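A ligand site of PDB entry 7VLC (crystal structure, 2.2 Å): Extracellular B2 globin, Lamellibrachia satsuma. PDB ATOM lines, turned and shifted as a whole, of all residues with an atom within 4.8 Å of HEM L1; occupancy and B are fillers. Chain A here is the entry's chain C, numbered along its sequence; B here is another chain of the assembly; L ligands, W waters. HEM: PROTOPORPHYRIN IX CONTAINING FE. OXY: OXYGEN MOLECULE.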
ATOM      1  N   LEU A  50      -2.033   4.011  21.353  1.00  0.00           N
ATOM      2  CA  LEU A  50      -2.373   2.593  21.237  1.00  0.00           C
ATOM      3  C   LEU A  50      -2.532   1.931  22.593  1.00  0.00           C
ATOM      4  O   LEU A  50      -3.157   0.866  22.675  1.00  0.00           O
ATOM      5  CB  LEU A  50      -1.313   1.870  20.410  1.00  0.00           C
ATOM      6  CG  LEU A  50      -1.211   2.315  18.958  1.00  0.00           C
ATOM      7  CD1 LEU A  50      -0.055   1.609  18.287  1.00  0.00           C
ATOM      8  CD2 LEU A  50      -2.522   2.035  18.236  1.00  0.00           C
ATOM      9  N   PHE A  51      -1.999   2.535  23.656  1.00  0.00           N
ATOM     10  CA  PHE A  51      -2.017   1.970  24.993  1.00  0.00           C
ATOM     11  C   PHE A  51      -2.863   2.810  25.941  1.00  0.00           C
ATOM     12  O   PHE A  51      -2.569   2.875  27.147  1.00  0.00           O
ATOM     13  CB  PHE A  51      -0.594   1.815  25.529  1.00  0.00           C
ATOM     14  CG  PHE A  51       0.346   1.138  24.568  1.00  0.00           C
ATOM     15  CD1 PHE A  51       1.074   1.870  23.656  1.00  0.00           C
ATOM     16  CD2 PHE A  51       0.483  -0.253  24.569  1.00  0.00           C
ATOM     17  CE1 PHE A  51       1.929   1.244  22.761  1.00  0.00           C
ATOM     18  CE2 PHE A  51       1.329  -0.878  23.686  1.00  0.00           C
ATOM     19  CZ  PHE A  51       2.057  -0.125  22.780  1.00  0.00           C
ATOM     20  N   ARG A  53      -5.637   2.075  27.111  1.00  0.00           N
ATOM     21  CA  ARG A  53      -6.270   1.213  28.093  1.00  0.00           C
ATOM     22  C   ARG A  53      -5.362   0.947  29.294  1.00  0.00           C
ATOM     23  O   ARG A  53      -5.866   0.776  30.410  1.00  0.00           O
ATOM     24  CB  ARG A  53      -6.672  -0.105  27.435  1.00  0.00           C
ATOM     25  CG  ARG A  53      -7.704  -0.897  28.210  1.00  0.00           C
ATOM     26  CD  ARG A  53      -7.779  -2.330  27.728  1.00  0.00           C
ATOM     27  NE  ARG A  53      -6.583  -3.082  28.087  1.00  0.00           N
ATOM     28  CZ  ARG A  53      -6.423  -3.705  29.242  1.00  0.00           C
ATOM     29  NH1 ARG A  53      -5.295  -4.370  29.493  1.00  0.00           N
ATOM     30  NH2 ARG A  53      -7.377  -3.678  30.167  1.00  0.00           N
ATOM     31  N   VAL A  54      -4.048   0.917  29.094  1.00  0.00           N
ATOM     32  CA  VAL A  54      -3.107   0.616  30.173  1.00  0.00           C
ATOM     33  C   VAL A  54      -2.376   1.873  30.636  1.00  0.00           C
ATOM     34  O   VAL A  54      -1.272   1.772  31.181  1.00  0.00           O
ATOM     35  CB  VAL A  54      -2.123  -0.490  29.755  1.00  0.00           C
ATOM     36  CG1 VAL A  54      -2.800  -1.858  29.838  1.00  0.00           C
ATOM     37  CG2 VAL A  54      -1.575  -0.225  28.358  1.00  0.00           C
ATOM     38  N   HIS A  67       1.197  -3.799  32.501  1.00  0.00           N
ATOM     39  CA  HIS A  67       1.331  -4.050  31.076  1.00  0.00           C
ATOM     40  C   HIS A  67       2.780  -4.316  30.692  1.00  0.00           C
ATOM     41  O   HIS A  67       3.071  -5.229  29.916  1.00  0.00           O
ATOM     42  CB  HIS A  67       0.780  -2.869  30.272  1.00  0.00           C
ATOM     43  CG  HIS A  67       1.154  -2.900  28.822  1.00  0.00           C
ATOM     44  ND1 HIS A  67       0.560  -3.751  27.915  1.00  0.00           N
ATOM     45  CD2 HIS A  67       2.076  -2.190  28.130  1.00  0.00           C
ATOM     46  CE1 HIS A  67       1.087  -3.549  26.718  1.00  0.00           C
ATOM     47  NE2 HIS A  67       2.012  -2.611  26.818  1.00  0.00           N
ATOM     48  N   ARG A  70       3.756  -7.715  31.517  1.00  0.00           N
ATOM     49  CA  ARG A  70       3.192  -8.699  30.588  1.00  0.00           C
ATOM     50  C   ARG A  70       3.981  -8.745  29.292  1.00  0.00           C
ATOM     51  O   ARG A  70       4.178  -9.814  28.702  1.00  0.00           O
ATOM     52  CB  ARG A  70       1.728  -8.397  30.311  1.00  0.00           C
ATOM     53  CG  ARG A  70       0.786  -8.708  31.469  1.00  0.00           C
ATOM     54  CD  ARG A  70      -0.669  -8.664  31.040  1.00  0.00           C
ATOM     55  NE  ARG A  70      -1.076  -7.343  30.559  1.00  0.00           N
ATOM     56  CZ  ARG A  70      -1.544  -6.379  31.344  1.00  0.00           C
ATOM     57  NH1 ARG A  70      -1.667  -6.576  32.641  1.00  0.00           N
ATOM     58  NH2 ARG A  70      -1.893  -5.210  30.819  1.00  0.00           N
ATOM     59  N   VAL A  71       4.445  -7.580  28.806  1.00  0.00           N
ATOM     60  CA  VAL A  71       5.206  -7.549  27.562  1.00  0.00           C
ATOM     61  C   VAL A  71       6.538  -8.263  27.728  1.00  0.00           C
ATOM     62  O   VAL A  71       6.941  -9.071  26.885  1.00  0.00           O
ATOM     63  CB  VAL A  71       5.390  -6.090  27.098  1.00  0.00           C
ATOM     64  CG1 VAL A  71       6.295  -6.037  25.879  1.00  0.00           C
ATOM     65  CG2 VAL A  71       4.041  -5.472  26.786  1.00  0.00           C
ATOM     66  N   GLY A  74       6.068 -11.933  27.995  1.00  0.00           N
ATOM     67  CA  GLY A  74       5.849 -12.526  26.686  1.00  0.00           C
ATOM     68  C   GLY A  74       7.126 -12.648  25.871  1.00  0.00           C
ATOM     69  O   GLY A  74       7.328 -13.641  25.175  1.00  0.00           O
ATOM     70  N   LEU A  75       7.990 -11.638  25.957  1.00  0.00           N
ATOM     71  CA  LEU A  75       9.281 -11.734  25.290  1.00  0.00           C
ATOM     72  C   LEU A  75      10.161 -12.796  25.939  1.00  0.00           C
ATOM     73  O   LEU A  75      10.897 -13.507  25.252  1.00  0.00           O
ATOM     74  CB  LEU A  75       9.971 -10.374  25.279  1.00  0.00           C
ATOM     75  CG  LEU A  75      11.324 -10.347  24.570  1.00  0.00           C
ATOM     76  CD1 LEU A  75      11.159 -10.666  23.080  1.00  0.00           C
ATOM     77  CD2 LEU A  75      12.043  -9.012  24.764  1.00  0.00           C
ATOM     78  N   LEU A  95       0.382 -14.659  20.293  1.00  0.00           N
ATOM     79  CA  LEU A  95       0.738 -13.254  20.439  1.00  0.00           C
ATOM     80  C   LEU A  95       0.268 -12.430  19.255  1.00  0.00           C
ATOM     81  O   LEU A  95      -0.095 -11.257  19.410  1.00  0.00           O
ATOM     82  CB  LEU A  95       2.252 -13.108  20.608  1.00  0.00           C
ATOM     83  CG  LEU A  95       2.868 -13.661  21.906  1.00  0.00           C
ATOM     84  CD1 LEU A  95       4.384 -13.644  21.841  1.00  0.00           C
ATOM     85  CD2 LEU A  95       2.366 -12.870  23.107  1.00  0.00           C
ATOM     86  N   GLN A  98      -3.311 -11.521  19.588  1.00  0.00           N
ATOM     87  CA  GLN A  98      -3.447 -10.542  20.658  1.00  0.00           C
ATOM     88  C   GLN A  98      -3.117  -9.138  20.181  1.00  0.00           C
ATOM     89  O   GLN A  98      -3.649  -8.159  20.726  1.00  0.00           O
ATOM     90  CB  GLN A  98      -2.561 -10.926  21.842  1.00  0.00           C
ATOM     91  CG  GLN A  98      -3.127 -12.032  22.714  1.00  0.00           C
ATOM     92  CD  GLN A  98      -2.229 -12.376  23.879  1.00  0.00           C
ATOM     93  OE1 GLN A  98      -1.000 -12.344  23.753  1.00  0.00           O
ATOM     94  NE2 GLN A  98      -2.825 -12.709  25.017  1.00  0.00           N
ATOM     95  N   HIS A  99      -2.255  -9.006  19.170  1.00  0.00           N
ATOM     96  CA  HIS A  99      -1.923  -7.712  18.579  1.00  0.00           C
ATOM     97  C   HIS A  99      -2.749  -7.422  17.330  1.00  0.00           C
ATOM     98  O   HIS A  99      -2.620  -6.346  16.747  1.00  0.00           O
ATOM     99  CB  HIS A  99      -0.426  -7.647  18.252  1.00  0.00           C
ATOM    100  CG  HIS A  99       0.448  -7.660  19.464  1.00  0.00           C
ATOM    101  ND1 HIS A  99       0.696  -8.799  20.194  1.00  0.00           N
ATOM    102  CD2 HIS A  99       1.130  -6.660  20.083  1.00  0.00           C
ATOM    103  CE1 HIS A  99       1.486  -8.507  21.211  1.00  0.00           C
ATOM    104  NE2 HIS A  99       1.759  -7.215  21.164  1.00  0.00           N
ATOM    105  N   ARG A 102      -6.452  -4.402  16.154  1.00  0.00           N
ATOM    106  CA  ARG A 102      -6.108  -3.157  16.845  1.00  0.00           C
ATOM    107  C   ARG A 102      -5.525  -2.220  15.795  1.00  0.00           C
ATOM    108  O   ARG A 102      -4.354  -2.358  15.411  1.00  0.00           O
ATOM    109  CB  ARG A 102      -5.123  -3.394  17.977  1.00  0.00           C
ATOM    110  CG  ARG A 102      -5.648  -4.283  19.091  1.00  0.00           C
ATOM    111  CD  ARG A 102      -4.596  -4.524  20.142  1.00  0.00           C
ATOM    112  NE  ARG A 102      -4.992  -5.555  21.097  1.00  0.00           N
ATOM    113  CZ  ARG A 102      -5.622  -5.319  22.242  1.00  0.00           C
ATOM    114  NH1 ARG A 102      -5.945  -6.323  23.047  1.00  0.00           N
ATOM    115  NH2 ARG A 102      -5.919  -4.076  22.591  1.00  0.00           N
ATOM    116  N   GLY A 104      -3.670   0.722  14.220  1.00  0.00           N
ATOM    117  CA  GLY A 104      -2.482   1.396  14.696  1.00  0.00           C
ATOM    118  C   GLY A 104      -1.339   0.476  15.062  1.00  0.00           C
ATOM    119  O   GLY A 104      -0.196   0.940  15.151  1.00  0.00           O
ATOM    120  N   VAL A 105      -1.624  -0.812  15.275  1.00  0.00           N
ATOM    121  CA  VAL A 105      -0.598  -1.798  15.579  1.00  0.00           C
ATOM    122  C   VAL A 105      -0.204  -2.450  14.247  1.00  0.00           C
ATOM    123  O   VAL A 105      -0.939  -3.281  13.708  1.00  0.00           O
ATOM    124  CB  VAL A 105      -1.084  -2.841  16.591  1.00  0.00           C
ATOM    125  CG1 VAL A 105       0.013  -3.851  16.878  1.00  0.00           C
ATOM    126  CG2 VAL A 105      -1.543  -2.155  17.866  1.00  0.00           C
ATOM    127  N   GLY A 109       5.504  -0.393  13.812  1.00  0.00           N
ATOM    128  CA  GLY A 109       5.733  -0.209  15.234  1.00  0.00           C
ATOM    129  C   GLY A 109       6.681  -1.241  15.825  1.00  0.00           C
ATOM    130  O   GLY A 109       7.416  -0.938  16.766  1.00  0.00           O
ATOM    131  N   PHE A 110       6.692  -2.452  15.259  1.00  0.00           N
ATOM    132  CA  PHE A 110       7.619  -3.473  15.739  1.00  0.00           C
ATOM    133  C   PHE A 110       9.043  -3.182  15.290  1.00  0.00           C
ATOM    134  O   PHE A 110       9.991  -3.423  16.038  1.00  0.00           O
ATOM    135  CB  PHE A 110       7.171  -4.852  15.253  1.00  0.00           C
ATOM    136  CG  PHE A 110       6.043  -5.437  16.058  1.00  0.00           C
ATOM    137  CD1 PHE A 110       4.741  -5.057  15.823  1.00  0.00           C
ATOM    138  CD2 PHE A 110       6.297  -6.357  17.066  1.00  0.00           C
ATOM    139  CE1 PHE A 110       3.698  -5.590  16.563  1.00  0.00           C
ATOM    140  CE2 PHE A 110       5.266  -6.888  17.815  1.00  0.00           C
ATOM    141  CZ  PHE A 110       3.961  -6.511  17.560  1.00  0.00           C
ATOM    142  N   ILE A 113      10.075  -0.576  17.901  1.00  0.00           N
ATOM    143  CA  ILE A 113      10.407  -1.121  19.211  1.00  0.00           C
ATOM    144  C   ILE A 113      11.649  -2.001  19.113  1.00  0.00           C
ATOM    145  O   ILE A 113      12.384  -2.151  20.094  1.00  0.00           O
ATOM    146  CB  ILE A 113       9.209  -1.892  19.803  1.00  0.00           C
ATOM    147  CG1 ILE A 113       9.327  -1.961  21.328  1.00  0.00           C
ATOM    148  CG2 ILE A 113       9.102  -3.295  19.217  1.00  0.00           C
ATOM    149  CD1 ILE A 113       8.140  -2.595  22.006  1.00  0.00           C
ATOM    150  N   PHE A 117      14.743  -1.618  21.707  1.00  0.00           N
ATOM    151  CA  PHE A 117      15.524  -2.633  22.404  1.00  0.00           C
ATOM    152  C   PHE A 117      17.016  -2.529  22.071  1.00  0.00           C
ATOM    153  O   PHE A 117      17.870  -2.732  22.940  1.00  0.00           O
ATOM    154  CB  PHE A 117      15.003  -4.026  22.076  1.00  0.00           C
ATOM    155  CG  PHE A 117      13.860  -4.483  22.932  1.00  0.00           C
ATOM    156  CD1 PHE A 117      14.090  -5.053  24.170  1.00  0.00           C
ATOM    157  CD2 PHE A 117      12.556  -4.339  22.493  1.00  0.00           C
ATOM    158  CE1 PHE A 117      13.034  -5.468  24.963  1.00  0.00           C
ATOM    159  CE2 PHE A 117      11.489  -4.757  23.278  1.00  0.00           C
ATOM    160  CZ  PHE A 117      11.728  -5.316  24.513  1.00  0.00           C
ATOM    161  N   PHE A 137      15.557 -11.487  17.516  1.00  0.00           N
ATOM    162  CA  PHE A 137      14.443 -10.610  17.821  1.00  0.00           C
ATOM    163  C   PHE A 137      13.532 -10.438  16.606  1.00  0.00           C
ATOM    164  O   PHE A 137      12.304 -10.469  16.741  1.00  0.00           O
ATOM    165  CB  PHE A 137      14.952  -9.245  18.299  1.00  0.00           C
ATOM    166  CG  PHE A 137      13.884  -8.336  18.828  1.00  0.00           C
ATOM    167  CD1 PHE A 137      13.204  -7.464  17.986  1.00  0.00           C
ATOM    168  CD2 PHE A 137      13.549  -8.358  20.178  1.00  0.00           C
ATOM    169  CE1 PHE A 137      12.218  -6.633  18.475  1.00  0.00           C
ATOM    170  CE2 PHE A 137      12.555  -7.514  20.686  1.00  0.00           C
ATOM    171  CZ  PHE A 137      11.893  -6.653  19.824  1.00  0.00           C
ATOM    172  N   THR A 141       9.582 -11.347  16.130  1.00  0.00           N
ATOM    173  CA  THR A 141       8.552 -10.420  15.652  1.00  0.00           C
ATOM    174  C   THR A 141       7.946 -10.851  14.323  1.00  0.00           C
ATOM    175  O   THR A 141       6.801 -10.478  14.045  1.00  0.00           O
ATOM    176  CB  THR A 141       9.117  -9.000  15.537  1.00  0.00           C
ATOM    177  OG1 THR A 141      10.182  -8.978  14.576  1.00  0.00           O
ATOM    178  CG2 THR A 141       9.627  -8.508  16.880  1.00  0.00           C
ATOM    179  N   MET A 144       4.994 -12.595  15.249  1.00  0.00           N
ATOM    180  CA  MET A 144       4.009 -11.755  15.921  1.00  0.00           C
ATOM    181  C   MET A 144       3.281 -10.816  14.962  1.00  0.00           C
ATOM    182  O   MET A 144       2.231 -10.277  15.327  1.00  0.00           O
ATOM    183  CB  MET A 144       4.678 -10.926  17.014  1.00  0.00           C
ATOM    184  CG  MET A 144       5.346 -11.738  18.114  1.00  0.00           C
ATOM    185  SD  MET A 144       5.989 -10.673  19.427  1.00  0.00           S
ATOM    186  CE  MET A 144       4.463  -9.986  20.076  1.00  0.00           C
ATOM    187  N   HIS B  90      -6.169  -8.731  35.804  1.00  0.00           N
ATOM    188  CA  HIS B  90      -6.045  -9.063  34.385  1.00  0.00           C
ATOM    189  C   HIS B  90      -6.225 -10.551  34.154  1.00  0.00           C
ATOM    190  O   HIS B  90      -6.874 -10.962  33.178  1.00  0.00           O
ATOM    191  CB  HIS B  90      -4.683  -8.597  33.863  1.00  0.00           C
ATOM    192  CG  HIS B  90      -4.546  -8.674  32.375  1.00  0.00           C
ATOM    193  ND1 HIS B  90      -4.884  -7.634  31.544  1.00  0.00           N
ATOM    194  CD2 HIS B  90      -4.107  -9.675  31.571  1.00  0.00           C
ATOM    195  CE1 HIS B  90      -4.659  -7.990  30.287  1.00  0.00           C
ATOM    196  NE2 HIS B  90      -4.183  -9.217  30.278  1.00  0.00           N
ATOM    197  N   GLN B  94      -9.274 -12.812  32.104  1.00  0.00           N
ATOM    198  CA  GLN B  94      -8.932 -13.851  31.137  1.00  0.00           C
ATOM    199  C   GLN B  94      -9.639 -15.169  31.431  1.00  0.00           C
ATOM    200  O   GLN B  94      -9.697 -16.031  30.546  1.00  0.00           O
ATOM    201  CB  GLN B  94      -7.417 -14.062  31.113  1.00  0.00           C
ATOM    202  CG  GLN B  94      -6.643 -12.872  30.544  1.00  0.00           C
ATOM    203  CD  GLN B  94      -5.134 -13.004  30.702  1.00  0.00           C
ATOM    204  OE1 GLN B  94      -4.644 -13.539  31.698  1.00  0.00           O
ATOM    205  NE2 GLN B  94      -4.384 -12.515  29.717  1.00  0.00           N
HETATM  206  CHA HEM L   1      -0.459  -6.216  24.578  1.00  0.00           C
HETATM  207  CHB HEM L   1       3.751  -8.573  23.943  1.00  0.00           C
HETATM  208  CHC HEM L   1       5.207  -5.165  20.805  1.00  0.00           C
HETATM  209  CHD HEM L   1       0.784  -3.146  21.020  1.00  0.00           C
HETATM  210  C1A HEM L   1       0.561  -7.139  24.708  1.00  0.00           C
HETATM  211  C2A HEM L   1       0.586  -8.277  25.616  1.00  0.00           C
HETATM  212  C3A HEM L   1       1.738  -8.917  25.428  1.00  0.00           C
HETATM  213  C4A HEM L   1       2.502  -8.217  24.413  1.00  0.00           C
HETATM  214  CMA HEM L   1       2.198 -10.198  26.181  1.00  0.00           C
HETATM  215  CAA HEM L   1      -0.525  -8.697  26.615  1.00  0.00           C
HETATM  216  CBA HEM L   1      -1.794  -9.116  25.880  1.00  0.00           C
HETATM  217  CGA HEM L   1      -2.795  -9.668  26.854  1.00  0.00           C
HETATM  218  O1A HEM L   1      -2.460  -9.823  28.052  1.00  0.00           O
HETATM  219  O2A HEM L   1      -3.949  -9.961  26.439  1.00  0.00           O
HETATM  220  C1B HEM L   1       4.527  -7.838  23.074  1.00  0.00           C
HETATM  221  C2B HEM L   1       5.898  -8.145  22.689  1.00  0.00           C
HETATM  222  C3B HEM L   1       6.306  -7.192  21.818  1.00  0.00           C
HETATM  223  C4B HEM L   1       5.204  -6.269  21.630  1.00  0.00           C
HETATM  224  CMB HEM L   1       6.684  -9.356  23.245  1.00  0.00           C
HETATM  225  CAB HEM L   1       7.662  -7.014  21.092  1.00  0.00           C
HETATM  226  CBB HEM L   1       8.674  -7.889  21.142  1.00  0.00           C
HETATM  227  C1C HEM L   1       4.137  -4.314  20.583  1.00  0.00           C
HETATM  228  C2C HEM L   1       4.129  -3.145  19.728  1.00  0.00           C
HETATM  229  C3C HEM L   1       2.911  -2.585  19.787  1.00  0.00           C
HETATM  230  C4C HEM L   1       2.106  -3.391  20.683  1.00  0.00           C
HETATM  231  CMC HEM L   1       5.371  -2.689  18.919  1.00  0.00           C
HETATM  232  CAC HEM L   1       2.357  -1.320  19.072  1.00  0.00           C
HETATM  233  CBC HEM L   1       3.052  -0.540  18.228  1.00  0.00           C
HETATM  234  C1D HEM L   1       0.070  -3.772  22.014  1.00  0.00           C
HETATM  235  C2D HEM L   1      -1.262  -3.417  22.477  1.00  0.00           C
HETATM  236  C3D HEM L   1      -1.599  -4.262  23.462  1.00  0.00           C
HETATM  237  C4D HEM L   1      -0.496  -5.183  23.660  1.00  0.00           C
HETATM  238  CMD HEM L   1      -2.133  -2.268  21.924  1.00  0.00           C
HETATM  239  CAD HEM L   1      -2.919  -4.283  24.246  1.00  0.00           C
HETATM  240  CBD HEM L   1      -2.908  -3.212  25.328  1.00  0.00           C
HETATM  241  CGD HEM L   1      -3.888  -3.581  26.410  1.00  0.00           C
HETATM  242  O1D HEM L   1      -4.349  -2.676  27.142  1.00  0.00           O
HETATM  243  O2D HEM L   1      -4.206  -4.795  26.532  1.00  0.00           O
HETATM  244  NA  HEM L   1       1.743  -7.133  23.998  1.00  0.00           N
HETATM  245  NB  HEM L   1       4.146  -6.697  22.405  1.00  0.00           N
HETATM  246  NC  HEM L   1       2.882  -4.443  21.151  1.00  0.00           N
HETATM  247  ND  HEM L   1       0.499  -4.855  22.758  1.00  0.00           N
HETATM  248 FE   HEM L   1       2.342  -5.808  22.558  1.00  0.00          FE
HETATM  249  O1  OXY L   2       3.014  -4.601  23.708  1.00  0.00           O
HETATM  250  O2  OXY L   2       2.755  -3.565  24.272  1.00  0.00           O
HETATM  251  O   HOH W   1       2.648 -12.012  28.984  1.00  0.00           O
HETATM  252  O   HOH W   2      -0.052 -11.546  28.787  1.00  0.00           O
HETATM  253  O   HOH W   3       2.774 -13.482  26.698  1.00  0.00           O
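An iron atom (FE) of HEM L1 is bound by a ring nitrogen (NE2) of His 99.
A ring nitrogen (NE2) of His 67 is in hydrogen-bond range of an oxygen (O2) of OXY L2 (2.8 Å).
NE2 of His 90 of chain B sits at hydrogen-bond distance from O1A of HEM L1 (2.9 Å).
An oxygen (O2A) of HEM L1 sits at hydrogen-bond distance from the side-chain amide nitrogen (NE2) of Gln 98.
The guanidinium group of Arg 53 lies within salt-bridge range of an oxygen (O1D) of HEM L1 (2.5 Å).
An oxygen (O1A) of HEM L1 lies within salt-bridge range of the guanidinium group (NE) of Arg 70 (3.8 Å).
FE of HEM L1 is bound by O1 of OXY L2 (1.8 Å).
NE of Arg 102 is in hydrogen-bond range of O of Gln 98 (3.0 Å).
The backbone carbonyl oxygen (O) of Phe 137 lies close to the side-chain hydroxyl (OG1) of Thr 141, 3.4 Å away.
NE2 of His 90 of chain B is in hydrogen-bond range of NE2 of Gln 94 of chain B (3.4 Å).
O of Leu 95 lies within hydrogen-bond range of ND1 of His 99 (2.7 Å).
Residues that only touch HEM L1: Val 54, Leu 50, Arg 102, Gly 109, Phe 110, Met 144, Phe 51, Val 71, Phe 137, Gln 94 of chain B, His 67, Leu 75 and Ile 113.
Hydrophobic or aromatic side chains within 4 Å of HEM L1: Leu 50, Phe 51, Val 54, His 67, Val 71, Leu 75, His 99, Phe 110, Ile 113, Phe 137, Met 144 and His 90 of chain B.
Within 4 Å of HEM L1: Leu 50, Phe 51, Arg 53, Val 54, His 67, Arg 70, Val 71, Leu 75, Gln 98, His 99, Arg 102, Gly 109, Phe 110, Ile 113, Phe 137, Met 144, His 90 of chain B and Gln 94 of chain B.
The nearest printed residue that does not touch HEM L1 is Val 105 (4.04 Å).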
